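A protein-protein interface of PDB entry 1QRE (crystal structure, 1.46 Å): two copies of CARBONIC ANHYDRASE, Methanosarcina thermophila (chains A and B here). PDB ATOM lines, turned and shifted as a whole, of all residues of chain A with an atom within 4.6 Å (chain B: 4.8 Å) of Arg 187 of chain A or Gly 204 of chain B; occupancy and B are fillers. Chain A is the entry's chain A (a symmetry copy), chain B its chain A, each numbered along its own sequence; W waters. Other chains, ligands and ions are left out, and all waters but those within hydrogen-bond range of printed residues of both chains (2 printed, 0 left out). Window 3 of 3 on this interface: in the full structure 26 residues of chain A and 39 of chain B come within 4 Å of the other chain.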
ATOM      1  N   MET A 169       6.988   1.975  29.473  1.00  0.00           N
ATOM      2  CA  MET A 169       7.751   1.780  28.240  1.00  0.00           C
ATOM      3  C   MET A 169       7.091   2.486  27.085  1.00  0.00           C
ATOM      4  O   MET A 169       5.877   2.369  26.869  1.00  0.00           O
ATOM      5  CB  MET A 169       7.944   0.295  27.894  1.00  0.00           C
ATOM      6  CG  MET A 169       8.654  -0.548  28.959  1.00  0.00           C
ATOM      7  SD  MET A 169       7.419  -1.129  30.187  1.00  0.00           S
ATOM      8  CE  MET A 169       8.286  -2.322  31.192  1.00  0.00           C
ATOM      9  N   GLN A 170       7.827   3.274  26.354  1.00  0.00           N
ATOM     10  CA  GLN A 170       7.381   3.973  25.146  1.00  0.00           C
ATOM     11  C   GLN A 170       6.325   5.027  25.444  1.00  0.00           C
ATOM     12  O   GLN A 170       5.731   5.534  24.485  1.00  0.00           O
ATOM     13  CB  GLN A 170       6.838   2.997  24.073  1.00  0.00           C
ATOM     14  CG  GLN A 170       7.941   2.125  23.470  1.00  0.00           C
ATOM     15  CD  GLN A 170       7.476   1.156  22.416  1.00  0.00           C
ATOM     16  OE1 GLN A 170       6.257   1.010  22.190  1.00  0.00           O
ATOM     17  NE2 GLN A 170       8.369   0.496  21.714  1.00  0.00           N
ATOM     18  N   ALA A 171       6.151   5.437  26.658  1.00  0.00           N
ATOM     19  CA  ALA A 171       5.171   6.463  27.031  1.00  0.00           C
ATOM     20  C   ALA A 171       5.675   7.849  26.712  1.00  0.00           C
ATOM     21  O   ALA A 171       6.890   8.057  26.517  1.00  0.00           O
ATOM     22  CB  ALA A 171       4.740   6.280  28.480  1.00  0.00           C
ATOM     23  N   GLU A 185       0.830   3.558  31.831  1.00  0.00           N
ATOM     24  CA  GLU A 185       1.110   2.238  31.260  1.00  0.00           C
ATOM     25  C   GLU A 185       1.904   2.398  29.966  1.00  0.00           C
ATOM     26  O   GLU A 185       1.970   3.487  29.397  1.00  0.00           O
ATOM     27  CB  GLU A 185      -0.239   1.534  31.023  1.00  0.00           C
ATOM     28  CG  GLU A 185      -0.868   1.085  32.347  1.00  0.00           C
ATOM     29  CD  GLU A 185      -2.094   0.201  32.132  1.00  0.00           C
ATOM     30  OE1 GLU A 185      -2.277  -0.353  31.044  1.00  0.00           O
ATOM     31  OE2 GLU A 185      -2.806   0.082  33.178  1.00  0.00           O
ATOM     32  N   PRO A 186       2.468   1.319  29.488  1.00  0.00           N
ATOM     33  CA  PRO A 186       3.232   1.372  28.240  1.00  0.00           C
ATOM     34  C   PRO A 186       2.435   1.998  27.134  1.00  0.00           C
ATOM     35  O   PRO A 186       1.200   1.801  27.004  1.00  0.00           O
ATOM     36  CB  PRO A 186       3.635  -0.083  27.920  1.00  0.00           C
ATOM     37  CG  PRO A 186       3.668  -0.662  29.306  1.00  0.00           C
ATOM     38  CD  PRO A 186       2.534  -0.006  30.110  1.00  0.00           C
ATOM     39  N   ARG A 187       3.011   2.875  26.327  1.00  0.00           N
ATOM     40  CA  ARG A 187       2.395   3.499  25.177  1.00  0.00           C
ATOM     41  C   ARG A 187       1.300   4.482  25.535  1.00  0.00           C
ATOM     42  O   ARG A 187       0.622   4.898  24.569  1.00  0.00           O
ATOM     43  CB  ARG A 187       1.888   2.402  24.224  1.00  0.00           C
ATOM     44  CG  ARG A 187       2.965   1.910  23.258  1.00  0.00           C
ATOM     45  CD  ARG A 187       3.055   2.926  22.125  1.00  0.00           C
ATOM     46  NE  ARG A 187       1.736   3.046  21.499  1.00  0.00           N
ATOM     47  CZ  ARG A 187       1.297   2.305  20.488  1.00  0.00           C
ATOM     48  NH1 ARG A 187       2.013   1.363  19.907  1.00  0.00           N
ATOM     49  NH2 ARG A 187       0.075   2.546  20.035  1.00  0.00           N
ATOM     50  N   SER A 188       1.169   4.881  26.772  1.00  0.00           N
ATOM     51  CA  SER A 188       0.177   5.915  27.108  1.00  0.00           C
ATOM     52  C   SER A 188       0.854   7.261  26.865  1.00  0.00           C
ATOM     53  O   SER A 188       2.115   7.395  26.736  1.00  0.00           O
ATOM     54  CB  SER A 188      -0.258   5.753  28.540  1.00  0.00           C
ATOM     55  OG  SER A 188       0.757   5.949  29.507  1.00  0.00           O
ATOM     56  N   ALA A 189       0.115   8.366  26.896  1.00  0.00           N
ATOM     57  CA  ALA A 189       0.666   9.700  26.721  1.00  0.00           C
ATOM     58  C   ALA A 189      -0.191  10.726  27.462  1.00  0.00           C
ATOM     59  O   ALA A 189      -1.424  10.537  27.533  1.00  0.00           O
ATOM     60  CB  ALA A 189       0.789  10.071  25.247  1.00  0.00           C
ATOM     61  N   GLY A 204      -1.700   2.575  25.761  1.00  0.00           N
ATOM     62  CA  GLY A 204      -2.035   3.087  24.452  1.00  0.00           C
ATOM     63  C   GLY A 204      -2.906   4.325  24.466  1.00  0.00           C
ATOM     64  O   GLY A 204      -3.010   4.946  23.382  1.00  0.00           O
ATOM     65  N   MET A 205      -3.440   4.756  25.605  1.00  0.00           N
ATOM     66  CA  MET A 205      -4.311   5.923  25.621  1.00  0.00           C
ATOM     67  C   MET A 205      -3.555   7.239  25.579  1.00  0.00           C
ATOM     68  O   MET A 205      -2.609   7.471  26.345  1.00  0.00           O
ATOM     69  CB  MET A 205      -5.222   5.823  26.859  1.00  0.00           C
ATOM     70  CG  MET A 205      -6.161   7.020  26.994  1.00  0.00           C
ATOM     71  SD  MET A 205      -7.111   6.975  28.535  1.00  0.00           S
ATOM     72  CE  MET A 205      -8.135   5.540  28.208  1.00  0.00           C
ATOM     73  N   GLN B 170       8.741   0.562  15.859  1.00  0.00           N
ATOM     74  CA  GLN B 170       8.117   1.193  17.024  1.00  0.00           C
ATOM     75  C   GLN B 170       7.113   0.278  17.710  1.00  0.00           C
ATOM     76  O   GLN B 170       6.381   0.773  18.575  1.00  0.00           O
ATOM     77  CB  GLN B 170       7.422   2.530  16.662  1.00  0.00           C
ATOM     78  CG  GLN B 170       8.427   3.623  16.289  1.00  0.00           C
ATOM     79  CD  GLN B 170       7.814   4.950  15.929  1.00  0.00           C
ATOM     80  OE1 GLN B 170       6.574   5.059  15.819  1.00  0.00           O
ATOM     81  NE2 GLN B 170       8.592   5.994  15.771  1.00  0.00           N
ATOM     82  N   PRO B 186       3.918  -1.842  12.207  1.00  0.00           N
ATOM     83  CA  PRO B 186       4.488  -0.699  12.926  1.00  0.00           C
ATOM     84  C   PRO B 186       3.533  -0.162  13.950  1.00  0.00           C
ATOM     85  O   PRO B 186       2.292  -0.112  13.747  1.00  0.00           O
ATOM     86  CB  PRO B 186       4.843   0.351  11.853  1.00  0.00           C
ATOM     87  CG  PRO B 186       5.086  -0.546  10.671  1.00  0.00           C
ATOM     88  CD  PRO B 186       4.083  -1.707  10.758  1.00  0.00           C
ATOM     89  N   ARG B 187       3.977   0.166  15.152  1.00  0.00           N
ATOM     90  CA  ARG B 187       3.193   0.764  16.212  1.00  0.00           C
ATOM     91  C   ARG B 187       2.161  -0.172  16.803  1.00  0.00           C
ATOM     92  O   ARG B 187       1.344   0.363  17.586  1.00  0.00           O
ATOM     93  CB  ARG B 187       2.554   2.063  15.686  1.00  0.00           C
ATOM     94  CG  ARG B 187       3.475   3.274  15.819  1.00  0.00           C
ATOM     95  CD  ARG B 187       3.391   3.752  17.264  1.00  0.00           C
ATOM     96  NE  ARG B 187       1.993   4.061  17.573  1.00  0.00           N
ATOM     97  CZ  ARG B 187       1.411   5.241  17.394  1.00  0.00           C
ATOM     98  NH1 ARG B 187       2.035   6.299  16.918  1.00  0.00           N
ATOM     99  NH2 ARG B 187       0.134   5.353  17.731  1.00  0.00           N
ATOM    100  N   SER B 188       2.216  -1.449  16.531  1.00  0.00           N
ATOM    101  CA  SER B 188       1.280  -2.378  17.185  1.00  0.00           C
ATOM    102  C   SER B 188       1.909  -2.753  18.525  1.00  0.00           C
ATOM    103  O   SER B 188       3.136  -2.547  18.804  1.00  0.00           O
ATOM    104  CB  SER B 188       1.065  -3.583  16.307  1.00  0.00           C
ATOM    105  OG  SER B 188       2.214  -4.379  16.082  1.00  0.00           O
ATOM    106  N   ALA B 189       1.179  -3.423  19.411  1.00  0.00           N
ATOM    107  CA  ALA B 189       1.692  -3.867  20.697  1.00  0.00           C
ATOM    108  C   ALA B 189       0.952  -5.122  21.156  1.00  0.00           C
ATOM    109  O   ALA B 189      -0.255  -5.246  20.862  1.00  0.00           O
ATOM    110  CB  ALA B 189       1.592  -2.770  21.754  1.00  0.00           C
ATOM    111  N   PRO B 202      -2.566  -5.340  13.200  1.00  0.00           N
ATOM    112  CA  PRO B 202      -2.651  -4.123  12.434  1.00  0.00           C
ATOM    113  C   PRO B 202      -1.879  -2.969  13.052  1.00  0.00           C
ATOM    114  O   PRO B 202      -1.836  -2.767  14.277  1.00  0.00           O
ATOM    115  CB  PRO B 202      -4.179  -3.806  12.295  1.00  0.00           C
ATOM    116  CG  PRO B 202      -4.765  -5.183  12.486  1.00  0.00           C
ATOM    117  CD  PRO B 202      -3.907  -5.942  13.480  1.00  0.00           C
ATOM    118  N   ALA B 203      -1.344  -2.069  12.209  1.00  0.00           N
ATOM    119  CA  ALA B 203      -0.614  -0.913  12.658  1.00  0.00           C
ATOM    120  C   ALA B 203      -1.383  -0.124  13.698  1.00  0.00           C
ATOM    121  O   ALA B 203      -2.592   0.152  13.576  1.00  0.00           O
ATOM    122  CB  ALA B 203      -0.301   0.066  11.536  1.00  0.00           C
ATOM    123  N   GLY B 204      -0.765   0.198  14.804  1.00  0.00           N
ATOM    124  CA  GLY B 204      -1.294   1.024  15.866  1.00  0.00           C
ATOM    125  C   GLY B 204      -2.156   0.286  16.865  1.00  0.00           C
ATOM    126  O   GLY B 204      -2.425   0.892  17.928  1.00  0.00           O
ATOM    127  N   MET B 205      -2.516  -0.976  16.638  1.00  0.00           N
ATOM    128  CA  MET B 205      -3.380  -1.681  17.575  1.00  0.00           C
ATOM    129  C   MET B 205      -2.644  -2.203  18.796  1.00  0.00           C
ATOM    130  O   MET B 205      -1.593  -2.854  18.694  1.00  0.00           O
ATOM    131  CB  MET B 205      -4.095  -2.810  16.810  1.00  0.00           C
ATOM    132  CG  MET B 205      -5.007  -3.641  17.707  1.00  0.00           C
ATOM    133  SD  MET B 205      -5.716  -5.064  16.838  1.00  0.00           S
ATOM    134  CE  MET B 205      -6.770  -4.199  15.674  1.00  0.00           C
ATOM    135  N   VAL B 206      -3.162  -1.907  19.971  1.00  0.00           N
ATOM    136  CA  VAL B 206      -2.610  -2.351  21.252  1.00  0.00           C
ATOM    137  C   VAL B 206      -3.460  -3.488  21.781  1.00  0.00           C
ATOM    138  O   VAL B 206      -4.634  -3.283  22.147  1.00  0.00           O
ATOM    139  CB  VAL B 206      -2.562  -1.173  22.238  1.00  0.00           C
ATOM    140  CG1 VAL B 206      -2.003  -1.634  23.573  1.00  0.00           C
ATOM    141  CG2 VAL B 206      -1.702  -0.040  21.682  1.00  0.00           C
HETATM  142  O   HOH W   1      -2.483   3.615  18.099  1.00  0.00           O
HETATM  143  O   HOH W   2       6.003   3.438  19.961  1.00  0.00           O
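The guanidinium group of Arg 187 of chain A sits at hydrogen-bond distance from the backbone carbonyl oxygen of Arg 187 of chain B (2.6 Å).
N of Gly 204 of chain B lies close to O of Arg 187 of chain B (3.5 Å). N of Gly 204 of chain A lies close to O of Arg 187 of chain A, at 3.5 Å. O of Pro 186 of chain B sits at hydrogen-bond distance from N of Gly 204 of chain B (3.2 Å). O of Met 169 of chain A is in hydrogen-bond range of N of Arg 187 of chain A.
Among the printed residues, pairs that only touch across the chains: Gln 170 of chain A with Gln 170 of chain B (3.6 Å), Arg 187 of chain A with Gly 204 of chain B (3.7 Å) and Arg 187 of chain A with Val 206 of chain B (3.5 Å).
Of the printed residues of chain B, Arg 187 of chain A touches Arg 187, Gly 204 and Val 206. Of the printed residues of chain A, Gly 204 of chain B touches Arg 187. Of the printed residues of chain A, Arg 187 of chain B touches Arg 187 (2.6 Å). Of the printed residues of chain A, Val 206 of chain B touches Arg 187 (3.5 Å). Printed residues of chain B within 4 Å of Gln 170 of chain A: Gln 170. The nearest printed residue of chain A that does not touch Gly 204 of chain B is Gly 204 of chain A (6.8 Å).
Hydrophobic or aromatic side chains of chain B within 4 Å of the printed part of chain A: Val 206. Among the printed residues, 4 pairs touch across the chains. Among the printed residues, no Asp or Glu carboxylate lies within 4 Å of a Lys or Arg side-chain nitrogen of the other chain.
Gln 170 of chain B touches its own counterpart, Gln 170 of chain A. Arg 187 of chain B touches its own counterpart, Arg 187 of chain A. Arg 187 of chain A touches Gly 204 of chain B, but with the chains exchanged Gly 204 of chain A does not touch Arg 187 of chain B (6.5 Å). Positions printed for both chains: 170, 186, 187, 188, 189, 204 and 205.
Water W1 lies within hydrogen-bond range of O of Gly 204 of chain B (2.7 Å), NH2 of Arg 187 of chain B (3.2 Å) and NH2 of Arg 187 of chain A (3.4 Å). Water W2 lies within hydrogen-bond range of the backbone carbonyl oxygen of Gln 170 of chain B (3.0 Å) and the side-chain amide oxygen of Gln 170 of chain A (3.3 Å).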
